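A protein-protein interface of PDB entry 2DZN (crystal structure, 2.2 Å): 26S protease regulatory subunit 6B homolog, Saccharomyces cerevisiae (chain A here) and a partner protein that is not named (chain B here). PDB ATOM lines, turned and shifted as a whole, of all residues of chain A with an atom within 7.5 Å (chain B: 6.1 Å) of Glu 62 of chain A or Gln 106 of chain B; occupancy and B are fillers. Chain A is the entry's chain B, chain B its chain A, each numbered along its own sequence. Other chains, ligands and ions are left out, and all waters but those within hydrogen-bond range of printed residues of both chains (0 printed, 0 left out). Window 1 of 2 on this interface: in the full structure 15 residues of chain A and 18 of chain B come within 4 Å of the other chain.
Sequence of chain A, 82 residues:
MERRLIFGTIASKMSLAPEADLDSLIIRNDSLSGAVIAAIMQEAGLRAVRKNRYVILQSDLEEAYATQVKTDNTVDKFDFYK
The side-chain carboxylate (OD1) of Asp 137 of chain B sits at hydrogen-bond distance from the backbone NH (N) of Phe 139 of chain B (2.9 Å). The side-chain hydroxyl of Thr 104 of chain B lies close to the backbone NH of Gln 106 of chain B, at 3.2 Å. The side-chain carboxylate (OE2) of Glu 62 of chain A is in salt-bridge range of the guanidinium group (NH2) of Arg 28 of chain A (2.8 Å). The side-chain hydroxyl (OG) of Ser 71 of chain B sits close to the indole nitrogen (NE1) of Trp 73 of chain B, 3.3 Å away. NE of Arg 28 of chain A sits at hydrogen-bond distance from O of Ser 24 of chain A (3.0 Å). The backbone carbonyl oxygen (O) of Gln 106 of chain B lies close to the backbone NH (N) of Lys 138 of chain B, 3.0 Å away.
Among the printed residues, pairs that only touch across the chains: Gln 58 of chain A with Trp 73 of chain B (3.0 Å), Arg 28 of chain A with Phe 139 of chain B (3.2 Å) and Glu 62 of chain A with Gln 106 of chain B (3.4 Å).
Printed residues of chain A that touch a printed residue of chain B: Arg 28, Gln 58 and Glu 62. Along chain A the printed residues that touch a printed residue of chain B span positions 28 to 62. Of the 11 printed residues of chain B, 3 touch a printed residue of chain A. Hydrophobic or aromatic side chains of chain B within 4 Å of the printed part of chain A: Trp 73 and Phe 139. Among the printed residues, 3 pairs touch across the chains.
Printed residues of chain B within 4 Å of Arg 28 of chain A: Phe 139. Of the printed residues of chain B, Gln 58 of chain A touches Trp 73 (3.0 Å). Ser 59 of chain A touches none of the printed residues of chain B. Glu 62 of chain A touches one residue of chain B. Printed residues of chain A within 4 Å of Trp 73 of chain B: Gln 58. Of chain A, only Glu 62 comes within 4 Å of Gln 106 of chain B. Printed residues of chain A within 4 Å of Phe 139 of chain B: Arg 28 (3.2 Å). The nearest residue of chain B that does not touch Glu 62 of chain A is Phe 139 of chain B (5.1 Å). The nearest residue of chain A that does not touch Gln 106 of chain B is Arg 28 of chain A (4.5 Å). The nearest printed residue of chain A that does not touch Trp 73 of chain B is Asp 21 of chain A (4.7 Å).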
ATOM      1  N   ASP A  21      17.068  -6.660  24.059  1.00  0.00           N
ATOM      2  CA  ASP A  21      16.914  -6.735  22.623  1.00  0.00           C
ATOM      3  C   ASP A  21      18.195  -6.378  21.870  1.00  0.00           C
ATOM      4  O   ASP A  21      18.318  -5.277  21.326  1.00  0.00           O
ATOM      5  CB  ASP A  21      15.774  -5.796  22.241  1.00  0.00           C
ATOM      6  CG  ASP A  21      15.468  -5.808  20.766  1.00  0.00           C
ATOM      7  OD1 ASP A  21      15.690  -6.857  20.114  1.00  0.00           O
ATOM      8  OD2 ASP A  21      14.985  -4.765  20.266  1.00  0.00           O
ATOM      9  N   LEU A  22      19.144  -7.316  21.858  1.00  0.00           N
ATOM     10  CA  LEU A  22      20.418  -7.144  21.170  1.00  0.00           C
ATOM     11  C   LEU A  22      20.201  -7.189  19.662  1.00  0.00           C
ATOM     12  O   LEU A  22      20.855  -6.467  18.906  1.00  0.00           O
ATOM     13  CB  LEU A  22      21.386  -8.248  21.574  1.00  0.00           C
ATOM     14  CG  LEU A  22      22.725  -8.316  20.847  1.00  0.00           C
ATOM     15  CD1 LEU A  22      23.526  -7.067  21.071  1.00  0.00           C
ATOM     16  CD2 LEU A  22      23.489  -9.505  21.368  1.00  0.00           C
ATOM     17  N   SER A  24      18.563  -5.781  17.730  1.00  0.00           N
ATOM     18  CA  SER A  24      17.874  -4.529  17.457  1.00  0.00           C
ATOM     19  C   SER A  24      18.997  -3.594  17.042  1.00  0.00           C
ATOM     20  O   SER A  24      18.837  -2.748  16.172  1.00  0.00           O
ATOM     21  CB  SER A  24      17.194  -4.001  18.729  1.00  0.00           C
ATOM     22  OG  SER A  24      17.277  -2.579  18.843  1.00  0.00           O
ATOM     23  N   LEU A  25      20.146  -3.768  17.678  1.00  0.00           N
ATOM     24  CA  LEU A  25      21.303  -2.953  17.366  1.00  0.00           C
ATOM     25  C   LEU A  25      21.890  -3.421  16.045  1.00  0.00           C
ATOM     26  O   LEU A  25      22.476  -2.640  15.296  1.00  0.00           O
ATOM     27  CB  LEU A  25      22.371  -3.092  18.447  1.00  0.00           C
ATOM     28  CG  LEU A  25      21.944  -2.992  19.904  1.00  0.00           C
ATOM     29  CD1 LEU A  25      23.193  -3.083  20.790  1.00  0.00           C
ATOM     30  CD2 LEU A  25      21.191  -1.705  20.121  1.00  0.00           C
ATOM     31  N   ARG A  28      20.159  -2.190  12.359  1.00  0.00           N
ATOM     32  CA  ARG A  28      20.300  -0.797  11.965  1.00  0.00           C
ATOM     33  C   ARG A  28      21.083  -0.453  10.728  1.00  0.00           C
ATOM     34  O   ARG A  28      20.514   0.024   9.752  1.00  0.00           O
ATOM     35  CB  ARG A  28      20.845  -0.008  13.140  1.00  0.00           C
ATOM     36  CG  ARG A  28      19.845   0.030  14.239  1.00  0.00           C
ATOM     37  CD  ARG A  28      20.442   0.470  15.528  1.00  0.00           C
ATOM     38  NE  ARG A  28      19.506   0.196  16.605  1.00  0.00           N
ATOM     39  CZ  ARG A  28      19.678   0.597  17.853  1.00  0.00           C
ATOM     40  NH1 ARG A  28      20.758   1.297  18.176  1.00  0.00           N
ATOM     41  NH2 ARG A  28      18.769   0.290  18.765  1.00  0.00           N
ATOM     42  N   ILE A  40      30.946  -3.477  21.562  1.00  0.00           N
ATOM     43  CA  ILE A  40      29.648  -3.080  22.103  1.00  0.00           C
ATOM     44  C   ILE A  40      29.271  -3.925  23.342  1.00  0.00           C
ATOM     45  O   ILE A  40      28.888  -3.379  24.380  1.00  0.00           O
ATOM     46  CB  ILE A  40      28.543  -3.257  21.040  1.00  0.00           C
ATOM     47  CG1 ILE A  40      28.787  -2.301  19.868  1.00  0.00           C
ATOM     48  CG2 ILE A  40      27.170  -3.039  21.659  1.00  0.00           C
ATOM     49  CD1 ILE A  40      27.852  -2.525  18.674  1.00  0.00           C
ATOM     50  N   ALA A  44      28.861  -2.701  27.076  1.00  0.00           N
ATOM     51  CA  ALA A  44      27.586  -2.823  27.777  1.00  0.00           C
ATOM     52  C   ALA A  44      27.846  -3.461  29.133  1.00  0.00           C
ATOM     53  O   ALA A  44      27.316  -3.014  30.146  1.00  0.00           O
ATOM     54  CB  ALA A  44      26.611  -3.673  26.979  1.00  0.00           C
ATOM     55  N   ARG A  47      29.071  -1.013  31.608  1.00  0.00           N
ATOM     56  CA  ARG A  47      28.029  -0.130  32.116  1.00  0.00           C
ATOM     57  C   ARG A  47      27.163  -0.796  33.188  1.00  0.00           C
ATOM     58  O   ARG A  47      26.699  -0.139  34.121  1.00  0.00           O
ATOM     59  CB  ARG A  47      27.162   0.383  30.965  1.00  0.00           C
ATOM     60  CG  ARG A  47      27.845   1.508  30.219  1.00  0.00           C
ATOM     61  CD  ARG A  47      27.338   1.734  28.817  1.00  0.00           C
ATOM     62  NE  ARG A  47      28.095   2.815  28.183  1.00  0.00           N
ATOM     63  CZ  ARG A  47      27.927   4.108  28.457  1.00  0.00           C
ATOM     64  NH1 ARG A  47      27.015   4.487  29.342  1.00  0.00           N
ATOM     65  NH2 ARG A  47      28.689   5.024  27.870  1.00  0.00           N
ATOM     66  N   ILE A  56      22.717  -7.404  31.901  1.00  0.00           N
ATOM     67  CA  ILE A  56      22.727  -6.301  30.950  1.00  0.00           C
ATOM     68  C   ILE A  56      21.323  -5.898  30.518  1.00  0.00           C
ATOM     69  O   ILE A  56      20.537  -6.747  30.112  1.00  0.00           O
ATOM     70  CB  ILE A  56      23.584  -6.698  29.708  1.00  0.00           C
ATOM     71  CG1 ILE A  56      25.046  -6.859  30.152  1.00  0.00           C
ATOM     72  CG2 ILE A  56      23.428  -5.684  28.575  1.00  0.00           C
ATOM     73  CD1 ILE A  56      25.982  -7.339  29.057  1.00  0.00           C
ATOM     74  N   LEU A  57      21.035  -4.596  30.608  1.00  0.00           N
ATOM     75  CA  LEU A  57      19.738  -4.003  30.226  1.00  0.00           C
ATOM     76  C   LEU A  57      19.870  -3.256  28.885  1.00  0.00           C
ATOM     77  O   LEU A  57      20.990  -2.961  28.443  1.00  0.00           O
ATOM     78  CB  LEU A  57      19.281  -3.020  31.304  1.00  0.00           C
ATOM     79  CG  LEU A  57      19.169  -3.569  32.735  1.00  0.00           C
ATOM     80  CD1 LEU A  57      18.728  -2.463  33.683  1.00  0.00           C
ATOM     81  CD2 LEU A  57      18.173  -4.713  32.786  1.00  0.00           C
ATOM     82  N   GLN A  58      18.738  -2.956  28.239  1.00  0.00           N
ATOM     83  CA  GLN A  58      18.747  -2.252  26.957  1.00  0.00           C
ATOM     84  C   GLN A  58      19.554  -0.971  26.970  1.00  0.00           C
ATOM     85  O   GLN A  58      20.192  -0.637  25.978  1.00  0.00           O
ATOM     86  CB  GLN A  58      17.327  -1.902  26.488  1.00  0.00           C
ATOM     87  CG  GLN A  58      16.682  -2.977  25.616  1.00  0.00           C
ATOM     88  CD  GLN A  58      17.512  -3.341  24.392  1.00  0.00           C
ATOM     89  OE1 GLN A  58      17.641  -2.564  23.441  1.00  0.00           O
ATOM     90  NE2 GLN A  58      18.085  -4.524  24.421  1.00  0.00           N
ATOM     91  N   SER A  59      19.507  -0.249  28.085  1.00  0.00           N
ATOM     92  CA  SER A  59      20.237   1.007  28.196  1.00  0.00           C
ATOM     93  C   SER A  59      21.715   0.762  28.000  1.00  0.00           C
ATOM     94  O   SER A  59      22.367   1.532  27.329  1.00  0.00           O
ATOM     95  CB  SER A  59      19.988   1.688  29.563  1.00  0.00           C
ATOM     96  OG  SER A  59      20.365   0.881  30.677  1.00  0.00           O
ATOM     97  N   ASP A  60      22.236  -0.317  28.574  1.00  0.00           N
ATOM     98  CA  ASP A  60      23.650  -0.604  28.425  1.00  0.00           C
ATOM     99  C   ASP A  60      23.937  -0.840  26.950  1.00  0.00           C
ATOM    100  O   ASP A  60      24.894  -0.278  26.416  1.00  0.00           O
ATOM    101  CB  ASP A  60      24.071  -1.833  29.233  1.00  0.00           C
ATOM    102  CG  ASP A  60      23.564  -1.804  30.672  1.00  0.00           C
ATOM    103  OD1 ASP A  60      23.470  -0.714  31.282  1.00  0.00           O
ATOM    104  OD2 ASP A  60      23.274  -2.896  31.202  1.00  0.00           O
ATOM    105  N   LEU A  61      23.097  -1.641  26.285  1.00  0.00           N
ATOM    106  CA  LEU A  61      23.291  -1.933  24.860  1.00  0.00           C
ATOM    107  C   LEU A  61      23.196  -0.701  23.942  1.00  0.00           C
ATOM    108  O   LEU A  61      24.035  -0.525  23.055  1.00  0.00           O
ATOM    109  CB  LEU A  61      22.279  -2.984  24.382  1.00  0.00           C
ATOM    110  CG  LEU A  61      22.363  -4.355  25.056  1.00  0.00           C
ATOM    111  CD1 LEU A  61      21.125  -5.159  24.703  1.00  0.00           C
ATOM    112  CD2 LEU A  61      23.641  -5.084  24.624  1.00  0.00           C
ATOM    113  N   GLU A  62      22.170   0.131  24.141  1.00  0.00           N
ATOM    114  CA  GLU A  62      21.963   1.329  23.321  1.00  0.00           C
ATOM    115  C   GLU A  62      23.093   2.339  23.536  1.00  0.00           C
ATOM    116  O   GLU A  62      23.533   2.999  22.599  1.00  0.00           O
ATOM    117  CB  GLU A  62      20.616   1.994  23.647  1.00  0.00           C
ATOM    118  CG  GLU A  62      19.377   1.177  23.304  1.00  0.00           C
ATOM    119  CD  GLU A  62      19.291   0.829  21.829  1.00  0.00           C
ATOM    120  OE1 GLU A  62      19.974   1.495  21.013  1.00  0.00           O
ATOM    121  OE2 GLU A  62      18.530  -0.103  21.485  1.00  0.00           O
ATOM    122  N   GLU A  63      23.546   2.463  24.776  1.00  0.00           N
ATOM    123  CA  GLU A  63      24.632   3.356  25.103  1.00  0.00           C
ATOM    124  C   GLU A  63      25.938   2.822  24.500  1.00  0.00           C
ATOM    125  O   GLU A  63      26.680   3.573  23.871  1.00  0.00           O
ATOM    126  CB  GLU A  63      24.751   3.494  26.624  1.00  0.00           C
ATOM    127  CG  GLU A  63      23.735   4.472  27.229  1.00  0.00           C
ATOM    128  CD  GLU A  63      23.408   4.162  28.680  1.00  0.00           C
ATOM    129  OE1 GLU A  63      24.273   3.573  29.381  1.00  0.00           O
ATOM    130  OE2 GLU A  63      22.291   4.517  29.120  1.00  0.00           O
ATOM    131  N   ALA A  64      26.203   1.532  24.676  1.00  0.00           N
ATOM    132  CA  ALA A  64      27.406   0.910  24.131  1.00  0.00           C
ATOM    133  C   ALA A  64      27.492   1.084  22.611  1.00  0.00           C
ATOM    134  O   ALA A  64      28.557   1.324  22.065  1.00  0.00           O
ATOM    135  CB  ALA A  64      27.429  -0.557  24.480  1.00  0.00           C
ATOM    136  N   TYR A  65      26.363   0.965  21.939  1.00  0.00           N
ATOM    137  CA  TYR A  65      26.300   1.128  20.494  1.00  0.00           C
ATOM    138  C   TYR A  65      26.546   2.597  20.107  1.00  0.00           C
ATOM    139  O   TYR A  65      27.297   2.895  19.169  1.00  0.00           O
ATOM    140  CB  TYR A  65      24.922   0.683  20.021  1.00  0.00           C
ATOM    141  CG  TYR A  65      24.618   0.907  18.560  1.00  0.00           C
ATOM    142  CD1 TYR A  65      25.042   0.000  17.589  1.00  0.00           C
ATOM    143  CD2 TYR A  65      23.863   2.010  18.152  1.00  0.00           C
ATOM    144  CE1 TYR A  65      24.717   0.178  16.243  1.00  0.00           C
ATOM    145  CE2 TYR A  65      23.537   2.201  16.812  1.00  0.00           C
ATOM    146  CZ  TYR A  65      23.967   1.280  15.864  1.00  0.00           C
ATOM    147  OH  TYR A  65      23.640   1.470  14.548  1.00  0.00           O
ATOM    148  N   ALA A  66      25.915   3.512  20.834  1.00  0.00           N
ATOM    149  CA  ALA A  66      26.059   4.932  20.550  1.00  0.00           C
ATOM    150  C   ALA A  66      27.517   5.406  20.534  1.00  0.00           C
ATOM    151  O   ALA A  66      27.809   6.477  20.006  1.00  0.00           O
ATOM    152  CB  ALA A  66      25.248   5.764  21.547  1.00  0.00           C
ATOM    153  N   THR A  67      28.429   4.621  21.101  1.00  0.00           N
ATOM    154  CA  THR A  67      29.835   5.014  21.100  1.00  0.00           C
ATOM    155  C   THR A  67      30.785   3.904  20.655  1.00  0.00           C
ATOM    156  O   THR A  67      31.812   3.654  21.287  1.00  0.00           O
ATOM    157  CB  THR A  67      30.289   5.525  22.488  1.00  0.00           C
ATOM    158  OG1 THR A  67      30.039   4.520  23.483  1.00  0.00           O
ATOM    159  CG2 THR A  67      29.544   6.816  22.849  1.00  0.00           C
ATOM    160  N   SER B  71      15.425   3.687  30.752  1.00  0.00           N
ATOM    161  CA  SER B  71      15.519   3.531  29.309  1.00  0.00           C
ATOM    162  C   SER B  71      14.194   3.840  28.626  1.00  0.00           C
ATOM    163  O   SER B  71      14.064   3.704  27.424  1.00  0.00           O
ATOM    164  CB  SER B  71      15.962   2.106  28.991  1.00  0.00           C
ATOM    165  OG  SER B  71      15.735   1.784  27.634  1.00  0.00           O
ATOM    166  N   TRP B  73      11.421   2.235  29.310  1.00  0.00           N
ATOM    167  CA  TRP B  73      10.611   1.011  29.242  1.00  0.00           C
ATOM    168  C   TRP B  73       9.670   0.894  30.431  1.00  0.00           C
ATOM    169  O   TRP B  73      10.105   0.898  31.582  1.00  0.00           O
ATOM    170  CB  TRP B  73      11.505  -0.234  29.235  1.00  0.00           C
ATOM    171  CG  TRP B  73      12.229  -0.507  27.976  1.00  0.00           C
ATOM    172  CD1 TRP B  73      12.964   0.386  27.233  1.00  0.00           C
ATOM    173  CD2 TRP B  73      12.408  -1.787  27.357  1.00  0.00           C
ATOM    174  NE1 TRP B  73      13.593  -0.266  26.206  1.00  0.00           N
ATOM    175  CE2 TRP B  73      13.274  -1.601  26.254  1.00  0.00           C
ATOM    176  CE3 TRP B  73      11.932  -3.078  27.636  1.00  0.00           C
ATOM    177  CZ2 TRP B  73      13.676  -2.659  25.421  1.00  0.00           C
ATOM    178  CZ3 TRP B  73      12.329  -4.128  26.816  1.00  0.00           C
ATOM    179  CH2 TRP B  73      13.199  -3.914  25.716  1.00  0.00           C
ATOM    180  N   ILE B 103       6.204   4.899  23.248  1.00  0.00           N
ATOM    181  CA  ILE B 103       7.536   4.566  22.781  1.00  0.00           C
ATOM    182  C   ILE B 103       8.587   4.665  23.873  1.00  0.00           C
ATOM    183  O   ILE B 103       8.431   5.405  24.834  1.00  0.00           O
ATOM    184  CB  ILE B 103       7.994   5.498  21.633  1.00  0.00           C
ATOM    185  CG1 ILE B 103       8.054   6.946  22.124  1.00  0.00           C
ATOM    186  CG2 ILE B 103       7.024   5.402  20.450  1.00  0.00           C
ATOM    187  CD1 ILE B 103       8.665   7.920  21.119  1.00  0.00           C
ATOM    188  N   THR B 104       9.653   3.894  23.718  1.00  0.00           N
ATOM    189  CA  THR B 104      10.773   3.919  24.635  1.00  0.00           C
ATOM    190  C   THR B 104      11.666   5.058  24.164  1.00  0.00           C
ATOM    191  O   THR B 104      11.366   5.728  23.168  1.00  0.00           O
ATOM    192  CB  THR B 104      11.577   2.639  24.536  1.00  0.00           C
ATOM    193  OG1 THR B 104      12.224   2.597  23.254  1.00  0.00           O
ATOM    194  CG2 THR B 104      10.661   1.431  24.695  1.00  0.00           C
ATOM    195  N   ASN B 105      12.786   5.255  24.848  1.00  0.00           N
ATOM    196  CA  ASN B 105      13.714   6.315  24.472  1.00  0.00           C
ATOM    197  C   ASN B 105      14.330   6.118  23.084  1.00  0.00           C
ATOM    198  O   ASN B 105      14.818   7.069  22.480  1.00  0.00           O
ATOM    199  CB  ASN B 105      14.797   6.452  25.550  1.00  0.00           C
ATOM    200  CG  ASN B 105      14.223   6.979  26.868  1.00  0.00           C
ATOM    201  OD1 ASN B 105      13.041   7.352  26.942  1.00  0.00           O
ATOM    202  ND2 ASN B 105      15.048   7.016  27.904  1.00  0.00           N
ATOM    203  N   GLN B 106      14.309   4.890  22.572  1.00  0.00           N
ATOM    204  CA  GLN B 106      14.830   4.624  21.242  1.00  0.00           C
ATOM    205  C   GLN B 106      13.673   4.701  20.265  1.00  0.00           C
ATOM    206  O   GLN B 106      13.822   4.402  19.076  1.00  0.00           O
ATOM    207  CB  GLN B 106      15.492   3.241  21.162  1.00  0.00           C
ATOM    208  CG  GLN B 106      16.915   3.228  21.697  1.00  0.00           C
ATOM    209  CD  GLN B 106      16.966   3.578  23.174  1.00  0.00           C
ATOM    210  OE1 GLN B 106      17.646   4.529  23.583  1.00  0.00           O
ATOM    211  NE2 GLN B 106      16.240   2.813  23.985  1.00  0.00           N
ATOM    212  N   GLY B 107      12.519   5.119  20.783  1.00  0.00           N
ATOM    213  CA  GLY B 107      11.334   5.231  19.959  1.00  0.00           C
ATOM    214  C   GLY B 107      10.629   3.920  19.598  1.00  0.00           C
ATOM    215  O   GLY B 107       9.802   3.929  18.689  1.00  0.00           O
ATOM    216  N   VAL B 108      10.913   2.813  20.282  1.00  0.00           N
ATOM    217  CA  VAL B 108      10.242   1.557  19.925  1.00  0.00           C
ATOM    218  C   VAL B 108       8.978   1.263  20.745  1.00  0.00           C
ATOM    219  O   VAL B 108       8.850   1.661  21.914  1.00  0.00           O
ATOM    220  CB  VAL B 108      11.191   0.309  20.014  1.00  0.00           C
ATOM    221  CG1 VAL B 108      12.531   0.594  19.288  1.00  0.00           C
ATOM    222  CG2 VAL B 108      11.414  -0.090  21.461  1.00  0.00           C
ATOM    223  N   ASP B 137      10.484   3.967  14.716  1.00  0.00           N
ATOM    224  CA  ASP B 137      11.421   4.194  15.822  1.00  0.00           C
ATOM    225  C   ASP B 137      12.542   5.143  15.383  1.00  0.00           C
ATOM    226  O   ASP B 137      12.474   5.719  14.298  1.00  0.00           O
ATOM    227  CB  ASP B 137      12.018   2.875  16.339  1.00  0.00           C
ATOM    228  CG  ASP B 137      12.833   2.118  15.278  1.00  0.00           C
ATOM    229  OD1 ASP B 137      13.222   2.699  14.228  1.00  0.00           O
ATOM    230  OD2 ASP B 137      13.093   0.918  15.516  1.00  0.00           O
ATOM    231  N   LYS B 138      13.574   5.297  16.206  1.00  0.00           N
ATOM    232  CA  LYS B 138      14.665   6.221  15.876  1.00  0.00           C
ATOM    233  C   LYS B 138      15.394   5.955  14.569  1.00  0.00           C
ATOM    234  O   LYS B 138      16.008   6.862  13.988  1.00  0.00           O
ATOM    235  CB  LYS B 138      15.681   6.281  17.014  1.00  0.00           C
ATOM    236  CG  LYS B 138      15.134   6.911  18.277  1.00  0.00           C
ATOM    237  CD  LYS B 138      14.573   8.302  18.020  1.00  0.00           C
ATOM    238  CE  LYS B 138      14.220   9.003  19.332  1.00  0.00           C
ATOM    239  NZ  LYS B 138      13.817  10.433  19.128  1.00  0.00           N
ATOM    240  N   PHE B 139      15.324   4.719  14.091  1.00  0.00           N
ATOM    241  CA  PHE B 139      15.991   4.379  12.846  1.00  0.00           C
ATOM    242  C   PHE B 139      15.008   4.289  11.697  1.00  0.00           C
ATOM    243  O   PHE B 139      15.357   3.862  10.603  1.00  0.00           O
ATOM    244  CB  PHE B 139      16.752   3.078  13.044  1.00  0.00           C
ATOM    245  CG  PHE B 139      17.807   3.182  14.093  1.00  0.00           C
ATOM    246  CD1 PHE B 139      19.106   3.559  13.758  1.00  0.00           C
ATOM    247  CD2 PHE B 139      17.489   2.981  15.434  1.00  0.00           C
ATOM    248  CE1 PHE B 139      20.082   3.741  14.754  1.00  0.00           C
ATOM    249  CE2 PHE B 139      18.444   3.162  16.423  1.00  0.00           C
ATOM    250  CZ  PHE B 139      19.745   3.542  16.084  1.00  0.00           C
